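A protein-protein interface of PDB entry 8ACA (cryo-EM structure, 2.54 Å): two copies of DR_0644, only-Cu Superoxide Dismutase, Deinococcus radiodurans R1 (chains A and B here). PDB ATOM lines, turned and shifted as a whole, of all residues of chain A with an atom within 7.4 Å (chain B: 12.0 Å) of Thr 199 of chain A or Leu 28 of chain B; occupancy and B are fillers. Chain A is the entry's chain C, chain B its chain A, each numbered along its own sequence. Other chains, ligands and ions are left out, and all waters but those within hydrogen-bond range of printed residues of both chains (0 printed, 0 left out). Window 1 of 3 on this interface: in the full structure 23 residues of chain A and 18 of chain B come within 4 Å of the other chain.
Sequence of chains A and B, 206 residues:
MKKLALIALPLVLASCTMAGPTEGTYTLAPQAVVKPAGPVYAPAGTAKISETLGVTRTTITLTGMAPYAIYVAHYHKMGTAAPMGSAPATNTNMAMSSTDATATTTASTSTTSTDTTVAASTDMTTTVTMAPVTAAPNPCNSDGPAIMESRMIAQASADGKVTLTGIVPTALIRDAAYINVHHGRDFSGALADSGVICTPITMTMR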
ATOM      1  N   PRO A  43      -7.398 -22.297 -20.091  1.00  0.00           N
ATOM      2  CA  PRO A  43      -8.545 -21.780 -20.826  1.00  0.00           C
ATOM      3  C   PRO A  43      -8.292 -21.517 -22.311  1.00  0.00           C
ATOM      4  O   PRO A  43      -7.285 -20.911 -22.624  1.00  0.00           O
ATOM      5  CB  PRO A  43      -8.884 -20.482 -20.092  1.00  0.00           C
ATOM      6  CG  PRO A  43      -8.368 -20.708 -18.697  1.00  0.00           C
ATOM      7  CD  PRO A  43      -7.094 -21.495 -18.906  1.00  0.00           C
ATOM      8  N   ALA A  44      -9.195 -21.998 -23.175  1.00  0.00           N
ATOM      9  CA  ALA A  44      -9.072 -21.810 -24.641  1.00  0.00           C
ATOM     10  C   ALA A  44     -10.420 -22.153 -25.287  1.00  0.00           C
ATOM     11  O   ALA A  44     -11.100 -23.060 -24.773  1.00  0.00           O
ATOM     12  CB  ALA A  44      -7.974 -22.693 -25.186  1.00  0.00           C
ATOM     13  N   GLY A  45     -10.737 -21.543 -26.438  1.00  0.00           N
ATOM     14  CA  GLY A  45     -11.974 -21.900 -27.168  1.00  0.00           C
ATOM     15  C   GLY A  45     -12.232 -20.992 -28.359  1.00  0.00           C
ATOM     16  O   GLY A  45     -11.267 -20.330 -28.773  1.00  0.00           O
ATOM     17  N   THR A  46     -13.491 -20.974 -28.854  1.00  0.00           N
ATOM     18  CA  THR A  46     -13.929 -20.163 -30.026  1.00  0.00           C
ATOM     19  C   THR A  46     -15.359 -19.635 -29.822  1.00  0.00           C
ATOM     20  O   THR A  46     -15.989 -20.061 -28.843  1.00  0.00           O
ATOM     21  CB  THR A  46     -13.968 -21.021 -31.289  1.00  0.00           C
ATOM     22  OG1 THR A  46     -14.465 -20.211 -32.355  1.00  0.00           O
ATOM     23  CG2 THR A  46     -14.840 -22.246 -31.129  1.00  0.00           C
ATOM     24  N   ALA A  47     -15.863 -18.755 -30.708  1.00  0.00           N
ATOM     25  CA  ALA A  47     -17.261 -18.271 -30.613  1.00  0.00           C
ATOM     26  C   ALA A  47     -17.907 -18.258 -32.004  1.00  0.00           C
ATOM     27  O   ALA A  47     -17.189 -17.967 -32.981  1.00  0.00           O
ATOM     28  CB  ALA A  47     -17.288 -16.900 -29.983  1.00  0.00           C
ATOM     29  N   LYS A  48     -19.207 -18.561 -32.085  1.00  0.00           N
ATOM     30  CA  LYS A  48     -19.940 -18.563 -33.378  1.00  0.00           C
ATOM     31  C   LYS A  48     -21.222 -17.747 -33.220  1.00  0.00           C
ATOM     32  O   LYS A  48     -22.285 -18.351 -33.033  1.00  0.00           O
ATOM     33  CB  LYS A  48     -20.291 -19.988 -33.808  1.00  0.00           C
ATOM     34  CG  LYS A  48     -19.104 -20.861 -34.194  1.00  0.00           C
ATOM     35  CD  LYS A  48     -19.495 -22.249 -34.660  1.00  0.00           C
ATOM     36  CE  LYS A  48     -20.072 -23.111 -33.559  1.00  0.00           C
ATOM     37  NZ  LYS A  48     -19.086 -23.362 -32.482  1.00  0.00           N
ATOM     38  N   THR A  59     -22.618 -19.471 -29.720  1.00  0.00           N
ATOM     39  CA  THR A  59     -22.181 -20.788 -29.183  1.00  0.00           C
ATOM     40  C   THR A  59     -20.694 -20.712 -28.818  1.00  0.00           C
ATOM     41  O   THR A  59     -19.863 -20.672 -29.747  1.00  0.00           O
ATOM     42  CB  THR A  59     -22.447 -21.917 -30.186  1.00  0.00           C
ATOM     43  OG1 THR A  59     -23.764 -21.752 -30.712  1.00  0.00           O
ATOM     44  CG2 THR A  59     -22.310 -23.292 -29.570  1.00  0.00           C
ATOM     45  N   ILE A  60     -20.381 -20.690 -27.517  1.00  0.00           N
ATOM     46  CA  ILE A  60     -18.960 -20.611 -27.073  1.00  0.00           C
ATOM     47  C   ILE A  60     -18.538 -21.981 -26.543  1.00  0.00           C
ATOM     48  O   ILE A  60     -18.840 -22.281 -25.370  1.00  0.00           O
ATOM     49  CB  ILE A  60     -18.729 -19.487 -26.046  1.00  0.00           C
ATOM     50  CG1 ILE A  60     -18.971 -18.105 -26.648  1.00  0.00           C
ATOM     51  CG2 ILE A  60     -17.329 -19.584 -25.465  1.00  0.00           C
ATOM     52  CD1 ILE A  60     -20.324 -17.546 -26.295  1.00  0.00           C
ATOM     53  N   THR A  61     -17.881 -22.782 -27.390  1.00  0.00           N
ATOM     54  CA  THR A  61     -17.369 -24.111 -26.958  1.00  0.00           C
ATOM     55  C   THR A  61     -15.965 -23.916 -26.379  1.00  0.00           C
ATOM     56  O   THR A  61     -15.073 -23.479 -27.135  1.00  0.00           O
ATOM     57  CB  THR A  61     -17.411 -25.127 -28.106  1.00  0.00           C
ATOM     58  OG1 THR A  61     -18.767 -25.286 -28.522  1.00  0.00           O
ATOM     59  CG2 THR A  61     -16.827 -26.469 -27.725  1.00  0.00           C
ATOM     60  N   LEU A  62     -15.790 -24.204 -25.085  1.00  0.00           N
ATOM     61  CA  LEU A  62     -14.480 -23.994 -24.412  1.00  0.00           C
ATOM     62  C   LEU A  62     -13.889 -25.347 -24.007  1.00  0.00           C
ATOM     63  O   LEU A  62     -14.679 -26.262 -23.711  1.00  0.00           O
ATOM     64  CB  LEU A  62     -14.701 -23.126 -23.171  1.00  0.00           C
ATOM     65  CG  LEU A  62     -15.105 -21.678 -23.435  1.00  0.00           C
ATOM     66  CD1 LEU A  62     -15.867 -21.110 -22.248  1.00  0.00           C
ATOM     67  CD2 LEU A  62     -13.888 -20.824 -23.744  1.00  0.00           C
ATOM     68  N   ALA A 177     -19.228  -4.928 -27.058  1.00  0.00           N
ATOM     69  CA  ALA A 177     -17.820  -4.857 -27.523  1.00  0.00           C
ATOM     70  C   ALA A 177     -17.103  -6.203 -27.383  1.00  0.00           C
ATOM     71  O   ALA A 177     -16.430  -6.609 -28.350  1.00  0.00           O
ATOM     72  CB  ALA A 177     -17.094  -3.775 -26.759  1.00  0.00           C
ATOM     73  N   TYR A 178     -17.231  -6.862 -26.230  1.00  0.00           N
ATOM     74  CA  TYR A 178     -16.463  -8.108 -25.997  1.00  0.00           C
ATOM     75  C   TYR A 178     -17.348  -9.125 -25.276  1.00  0.00           C
ATOM     76  O   TYR A 178     -17.986  -8.763 -24.276  1.00  0.00           O
ATOM     77  CB  TYR A 178     -15.129  -7.808 -25.307  1.00  0.00           C
ATOM     78  CG  TYR A 178     -15.195  -7.217 -23.924  1.00  0.00           C
ATOM     79  CD1 TYR A 178     -15.455  -5.871 -23.722  1.00  0.00           C
ATOM     80  CD2 TYR A 178     -14.956  -8.006 -22.814  1.00  0.00           C
ATOM     81  CE1 TYR A 178     -15.503  -5.330 -22.450  1.00  0.00           C
ATOM     82  CE2 TYR A 178     -15.000  -7.481 -21.536  1.00  0.00           C
ATOM     83  CZ  TYR A 178     -15.270  -6.139 -21.353  1.00  0.00           C
ATOM     84  OH  TYR A 178     -15.319  -5.637 -20.088  1.00  0.00           O
ATOM     85  N   ILE A 179     -17.400 -10.361 -25.787  1.00  0.00           N
ATOM     86  CA  ILE A 179     -18.134 -11.433 -25.052  1.00  0.00           C
ATOM     87  C   ILE A 179     -17.191 -11.890 -23.937  1.00  0.00           C
ATOM     88  O   ILE A 179     -16.132 -12.470 -24.256  1.00  0.00           O
ATOM     89  CB  ILE A 179     -18.548 -12.597 -25.975  1.00  0.00           C
ATOM     90  CG1 ILE A 179     -19.803 -12.265 -26.783  1.00  0.00           C
ATOM     91  CG2 ILE A 179     -18.738 -13.883 -25.183  1.00  0.00           C
ATOM     92  CD1 ILE A 179     -20.375 -13.451 -27.521  1.00  0.00           C
ATOM     93  N   ASN A 180     -17.531 -11.579 -22.686  1.00  0.00           N
ATOM     94  CA  ASN A 180     -16.638 -11.923 -21.551  1.00  0.00           C
ATOM     95  C   ASN A 180     -17.179 -13.170 -20.852  1.00  0.00           C
ATOM     96  O   ASN A 180     -18.335 -13.126 -20.388  1.00  0.00           O
ATOM     97  CB  ASN A 180     -16.452 -10.745 -20.593  1.00  0.00           C
ATOM     98  CG  ASN A 180     -15.175 -10.843 -19.785  1.00  0.00           C
ATOM     99  OD1 ASN A 180     -14.399 -11.780 -19.953  1.00  0.00           O
ATOM    100  ND2 ASN A 180     -14.949  -9.879 -18.908  1.00  0.00           N
ATOM    101  N   VAL A 181     -16.386 -14.245 -20.805  1.00  0.00           N
ATOM    102  CA  VAL A 181     -16.830 -15.444 -20.038  1.00  0.00           C
ATOM    103  C   VAL A 181     -16.353 -15.229 -18.611  1.00  0.00           C
ATOM    104  O   VAL A 181     -15.259 -14.682 -18.447  1.00  0.00           O
ATOM    105  CB  VAL A 181     -16.232 -16.739 -20.615  1.00  0.00           C
ATOM    106  CG1 VAL A 181     -16.574 -17.957 -19.775  1.00  0.00           C
ATOM    107  CG2 VAL A 181     -16.656 -16.950 -22.058  1.00  0.00           C
ATOM    108  N   ILE A 197     -11.909 -15.520 -19.492  1.00  0.00           N
ATOM    109  CA  ILE A 197     -11.531 -15.497 -20.936  1.00  0.00           C
ATOM    110  C   ILE A 197     -12.472 -14.516 -21.650  1.00  0.00           C
ATOM    111  O   ILE A 197     -13.644 -14.435 -21.243  1.00  0.00           O
ATOM    112  CB  ILE A 197     -11.550 -16.926 -21.525  1.00  0.00           C
ATOM    113  CG1 ILE A 197     -10.780 -17.031 -22.841  1.00  0.00           C
ATOM    114  CG2 ILE A 197     -12.960 -17.477 -21.655  1.00  0.00           C
ATOM    115  CD1 ILE A 197      -9.944 -18.281 -22.957  1.00  0.00           C
ATOM    116  N   CYS A 198     -11.970 -13.764 -22.635  1.00  0.00           N
ATOM    117  CA  CYS A 198     -12.803 -12.736 -23.310  1.00  0.00           C
ATOM    118  C   CYS A 198     -12.448 -12.667 -24.793  1.00  0.00           C
ATOM    119  O   CYS A 198     -11.255 -12.736 -25.112  1.00  0.00           O
ATOM    120  CB  CYS A 198     -12.486 -11.362 -22.761  1.00  0.00           C
ATOM    121  SG  CYS A 198     -10.761 -10.884 -23.038  1.00  0.00           S
ATOM    122  N   THR A 199     -13.450 -12.513 -25.666  1.00  0.00           N
ATOM    123  CA  THR A 199     -13.191 -12.416 -27.130  1.00  0.00           C
ATOM    124  C   THR A 199     -13.697 -11.077 -27.691  1.00  0.00           C
ATOM    125  O   THR A 199     -14.862 -10.741 -27.399  1.00  0.00           O
ATOM    126  CB  THR A 199     -13.772 -13.607 -27.904  1.00  0.00           C
ATOM    127  OG1 THR A 199     -13.595 -13.329 -29.292  1.00  0.00           O
ATOM    128  CG2 THR A 199     -15.233 -13.866 -27.613  1.00  0.00           C
ATOM    129  N   PRO A 200     -12.911 -10.273 -28.457  1.00  0.00           N
ATOM    130  CA  PRO A 200     -13.439  -9.052 -29.081  1.00  0.00           C
ATOM    131  C   PRO A 200     -14.497  -9.350 -30.152  1.00  0.00           C
ATOM    132  O   PRO A 200     -14.208 -10.088 -31.065  1.00  0.00           O
ATOM    133  CB  PRO A 200     -12.237  -8.392 -29.770  1.00  0.00           C
ATOM    134  CG  PRO A 200     -11.226  -9.496 -29.930  1.00  0.00           C
ATOM    135  CD  PRO A 200     -11.452 -10.379 -28.725  1.00  0.00           C
ATOM    136  N   ILE A 201     -15.676  -8.725 -30.036  1.00  0.00           N
ATOM    137  CA  ILE A 201     -16.800  -8.976 -30.991  1.00  0.00           C
ATOM    138  C   ILE A 201     -16.898  -7.811 -31.983  1.00  0.00           C
ATOM    139  O   ILE A 201     -17.294  -8.082 -33.135  1.00  0.00           O
ATOM    140  CB  ILE A 201     -18.132  -9.185 -30.242  1.00  0.00           C
ATOM    141  CG1 ILE A 201     -18.765  -7.863 -29.802  1.00  0.00           C
ATOM    142  CG2 ILE A 201     -17.941 -10.138 -29.073  1.00  0.00           C
ATOM    143  CD1 ILE A 201     -19.838  -7.354 -30.733  1.00  0.00           C
ATOM    144  N   GLU B  23     -22.995 -14.900 -40.237  1.00  0.00           N
ATOM    145  CA  GLU B  23     -22.287 -15.803 -39.294  1.00  0.00           C
ATOM    146  C   GLU B  23     -21.232 -15.026 -38.497  1.00  0.00           C
ATOM    147  O   GLU B  23     -21.419 -13.817 -38.300  1.00  0.00           O
ATOM    148  CB  GLU B  23     -21.710 -16.993 -40.058  1.00  0.00           C
ATOM    149  CG  GLU B  23     -22.727 -17.717 -40.923  1.00  0.00           C
ATOM    150  CD  GLU B  23     -23.514 -18.815 -40.228  1.00  0.00           C
ATOM    151  OE1 GLU B  23     -24.389 -18.489 -39.409  1.00  0.00           O
ATOM    152  OE2 GLU B  23     -23.253 -19.996 -40.519  1.00  0.00           O
ATOM    153  N   GLY B  24     -20.174 -15.715 -38.051  1.00  0.00           N
ATOM    154  CA  GLY B  24     -19.096 -15.113 -37.238  1.00  0.00           C
ATOM    155  C   GLY B  24     -18.397 -16.211 -36.452  1.00  0.00           C
ATOM    156  O   GLY B  24     -19.105 -17.120 -36.030  1.00  0.00           O
ATOM    157  N   THR B  25     -17.065 -16.150 -36.333  1.00  0.00           N
ATOM    158  CA  THR B  25     -16.276 -17.166 -35.581  1.00  0.00           C
ATOM    159  C   THR B  25     -15.117 -16.444 -34.888  1.00  0.00           C
ATOM    160  O   THR B  25     -14.340 -15.778 -35.605  1.00  0.00           O
ATOM    161  CB  THR B  25     -15.766 -18.276 -36.510  1.00  0.00           C
ATOM    162  OG1 THR B  25     -16.892 -18.964 -37.058  1.00  0.00           O
ATOM    163  CG2 THR B  25     -14.863 -19.267 -35.808  1.00  0.00           C
ATOM    164  N   TYR B  26     -15.024 -16.527 -33.559  1.00  0.00           N
ATOM    165  CA  TYR B  26     -13.968 -15.783 -32.824  1.00  0.00           C
ATOM    166  C   TYR B  26     -13.250 -16.745 -31.874  1.00  0.00           C
ATOM    167  O   TYR B  26     -13.932 -17.374 -31.041  1.00  0.00           O
ATOM    168  CB  TYR B  26     -14.576 -14.598 -32.065  1.00  0.00           C
ATOM    169  CG  TYR B  26     -15.172 -13.526 -32.943  1.00  0.00           C
ATOM    170  CD1 TYR B  26     -14.393 -12.495 -33.441  1.00  0.00           C
ATOM    171  CD2 TYR B  26     -16.515 -13.544 -33.284  1.00  0.00           C
ATOM    172  CE1 TYR B  26     -14.930 -11.510 -34.252  1.00  0.00           C
ATOM    173  CE2 TYR B  26     -17.068 -12.567 -34.095  1.00  0.00           C
ATOM    174  CZ  TYR B  26     -16.274 -11.545 -34.581  1.00  0.00           C
ATOM    175  OH  TYR B  26     -16.812 -10.577 -35.379  1.00  0.00           O
ATOM    176  N   THR B  27     -11.919 -16.822 -31.947  1.00  0.00           N
ATOM    177  CA  THR B  27     -11.131 -17.674 -31.013  1.00  0.00           C
ATOM    178  C   THR B  27     -10.987 -16.932 -29.681  1.00  0.00           C
ATOM    179  O   THR B  27     -11.035 -15.692 -29.700  1.00  0.00           O
ATOM    180  CB  THR B  27      -9.784 -18.064 -31.628  1.00  0.00           C
ATOM    181  OG1 THR B  27     -10.044 -18.660 -32.897  1.00  0.00           O
ATOM    182  CG2 THR B  27      -8.997 -19.025 -30.765  1.00  0.00           C
ATOM    183  N   LEU B  28     -10.806 -17.654 -28.570  1.00  0.00           N
ATOM    184  CA  LEU B  28     -10.817 -16.948 -27.250  1.00  0.00           C
ATOM    185  C   LEU B  28      -9.434 -16.441 -26.812  1.00  0.00           C
ATOM    186  O   LEU B  28      -8.428 -17.003 -27.287  1.00  0.00           O
ATOM    187  CB  LEU B  28     -11.415 -17.885 -26.194  1.00  0.00           C
ATOM    188  CG  LEU B  28     -12.940 -17.876 -26.102  1.00  0.00           C
ATOM    189  CD1 LEU B  28     -13.457 -16.473 -25.825  1.00  0.00           C
ATOM    190  CD2 LEU B  28     -13.563 -18.433 -27.371  1.00  0.00           C
ATOM    191  N   ALA B  29      -9.398 -15.423 -25.945  1.00  0.00           N
ATOM    192  CA  ALA B  29      -8.124 -14.917 -25.378  1.00  0.00           C
ATOM    193  C   ALA B  29      -8.341 -14.800 -23.868  1.00  0.00           C
ATOM    194  O   ALA B  29      -9.270 -14.076 -23.471  1.00  0.00           O
ATOM    195  CB  ALA B  29      -7.778 -13.584 -25.993  1.00  0.00           C
ATOM    196  N   PRO B  30      -7.523 -15.412 -22.967  1.00  0.00           N
ATOM    197  CA  PRO B  30      -7.810 -15.374 -21.521  1.00  0.00           C
ATOM    198  C   PRO B  30      -7.431 -14.083 -20.775  1.00  0.00           C
ATOM    199  O   PRO B  30      -6.885 -14.204 -19.691  1.00  0.00           O
ATOM    200  CB  PRO B  30      -6.999 -16.555 -20.968  1.00  0.00           C
ATOM    201  CG  PRO B  30      -5.779 -16.599 -21.856  1.00  0.00           C
ATOM    202  CD  PRO B  30      -6.279 -16.176 -23.221  1.00  0.00           C
ATOM    203  N   GLN B  31      -7.725 -12.906 -21.345  1.00  0.00           N
ATOM    204  CA  GLN B  31      -7.462 -11.597 -20.676  1.00  0.00           C
ATOM    205  C   GLN B  31      -5.997 -11.475 -20.240  1.00  0.00           C
ATOM    206  O   GLN B  31      -5.131 -12.101 -20.886  1.00  0.00           O
ATOM    207  CB  GLN B  31      -8.363 -11.411 -19.452  1.00  0.00           C
ATOM    208  CG  GLN B  31      -9.843 -11.618 -19.727  1.00  0.00           C
ATOM    209  CD  GLN B  31     -10.695 -10.614 -18.990  1.00  0.00           C
ATOM    210  OE1 GLN B  31     -11.700 -10.127 -19.502  1.00  0.00           O
ATOM    211  NE2 GLN B  31     -10.295 -10.298 -17.769  1.00  0.00           N
ATOM    212  N   ALA B  32      -5.727 -10.661 -19.211  1.00  0.00           N
ATOM    213  CA  ALA B  32      -4.355 -10.547 -18.666  1.00  0.00           C
ATOM    214  C   ALA B  32      -4.422 -10.914 -17.182  1.00  0.00           C
ATOM    215  O   ALA B  32      -3.599 -11.738 -16.737  1.00  0.00           O
ATOM    216  CB  ALA B  32      -3.832  -9.148 -18.868  1.00  0.00           C
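N of Lys 48 of chain A is in hydrogen-bond range of O of Thr 59 of chain A, at 3.2 Å. The backbone NH (N) of Val 181 of chain A sits at hydrogen-bond distance from the backbone carbonyl oxygen (O) of Ile 197 of chain A, at 2.8 Å. The backbone carbonyl oxygen of Ala 177 of chain A lies within hydrogen-bond range of the backbone NH of Ile 201 of chain A (2.8 Å). The backbone carbonyl oxygen of Ile 179 of chain A is in hydrogen-bond range of the backbone NH of Thr 199 of chain A, at 3.0 Å. The backbone carbonyl oxygen (O) of Ile 197 of chain A lies close to the side-chain amide oxygen (OD1) of Asn 180 of chain A, at 3.0 Å. The backbone NH (N) of Thr 46 of chain A lies within hydrogen-bond range of the backbone carbonyl oxygen (O) of Thr 61 of chain A.
The backbone carbonyl oxygen (O) of Gly 45 of chain A lies within hydrogen-bond range of the backbone NH (N) of Leu 28 of chain B. O of Ala 29 of chain B lies within hydrogen-bond range of N of Cys 198 of chain A (2.8 Å). OE1 of Gln 31 of chain B sits close to SG of Cys 198 of chain A, 3.7 Å away. O of Ala 47 of chain A lies within hydrogen-bond range of N of Tyr 26 of chain B (2.7 Å). The backbone carbonyl oxygen of Tyr 26 of chain B sits close to the side-chain hydroxyl of Thr 46 of chain A, at 3.2 Å. The side-chain amide oxygen (OE1) of Gln 31 of chain B lies close to the side-chain amide oxygen (OD1) of Asn 180 of chain A. The side-chain hydroxyl of Tyr 26 of chain B sits at hydrogen-bond distance from the backbone carbonyl oxygen of Ile 201 of chain A (3.4 Å).
Hydrophobic or aromatic side chains of chain A that line the printed part of chain B: Ala 47, Leu 62 and Ile 197. Among the printed residues, 22 pairs touch across the chains.
Among the printed residues, merely in contact across the chains: Gly 45 of chain A with Thr 27 of chain B (3.3 Å), Thr 46 of chain A with Thr 25 of chain B (3.6 Å), Thr 46 of chain A with Thr 27 of chain B (3.9 Å), Thr 46 of chain A with Leu 28 of chain B (2.9 Å), Ala 47 of chain A with Gly 24 of chain B (3.7 Å), Ala 47 of chain A with Thr 25 of chain B (2.9 Å), Lys 48 of chain A with Gly 24 of chain B (3.1 Å), Leu 62 of chain A with Leu 28 of chain B (3.9 Å), Ile 197 of chain A with Leu 28 of chain B (3.5 Å), Ile 197 of chain A with Ala 29 of chain B (3.4 Å), Ile 197 of chain A with Pro 30 of chain B (3.6 Å), Thr 199 of chain A with Tyr 26 of chain B (3.2 Å), Thr 199 of chain A with Thr 27 of chain B (3.5 Å), Thr 199 of chain A with Leu 28 of chain B (3.6 Å) and Pro 200 of chain A with Tyr 26 of chain B (3.4 Å).
No position is printed for both chains. Of the 22 pairs that touch across the chains among the printed residues, none has its exchanged pair printed and touching as well.
Of chain B, only Thr 27 and Leu 28 come within 4 Å of Gly 45 of chain A. Of chain B, only Thr 25 (3.6 Å), Tyr 26 (2.9 Å), Thr 27 (3.9 Å) and Leu 28 (2.9 Å) come within 4 Å of Thr 46 of chain A. Thr 59 of chain A touches none of the printed residues of chain B. No residue of chain B comes within 4 Å of Ile 60 of chain A. No residue of chain B comes within 4 Å of Ala 177 of chain A. No residue of chain B comes within 4 Å of Ile 179 of chain A. No residue of chain B comes within 4 Å of Val 181 of chain A. Of chain B, only Ala 29 and Gln 31 come within 4 Å of Cys 198 of chain A. Thr 199 of chain A touches just these residues of chain B: Tyr 26 (3.2 Å), Thr 27 (3.5 Å) and Leu 28 (3.6 Å). Of chain B, only Tyr 26 comes within 4 Å of Ile 201 of chain A. Of the printed residues of chain A, Gly 24 of chain B touches Ala 47 (3.7 Å) and Lys 48 (3.1 Å). Of chain A, only Gly 45, Thr 46, Leu 62, Ile 197 and Thr 199 come within 4 Å of Leu 28 of chain B. Of the printed residues of chain A, Ala 29 of chain B touches Ile 197 (3.4 Å) and Cys 198 (2.8 Å). Of the printed residues of chain A, Pro 30 of chain B touches Ile 197 (3.6 Å). Of the printed residues of chain A, Gln 31 of chain B touches Asn 180 (3.2 Å) and Cys 198 (3.5 Å). The nearest residue of chain B that does not touch Thr 199 of chain A is Ala 29 of chain B (5.0 Å). The nearest printed residue of chain A that does not touch Leu 28 of chain B is Ala 47 of chain A (4.1 Å). The nearest printed residue of chain A that does not touch Thr 27 of chain B is Ala 47 of chain A (4.6 Å).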
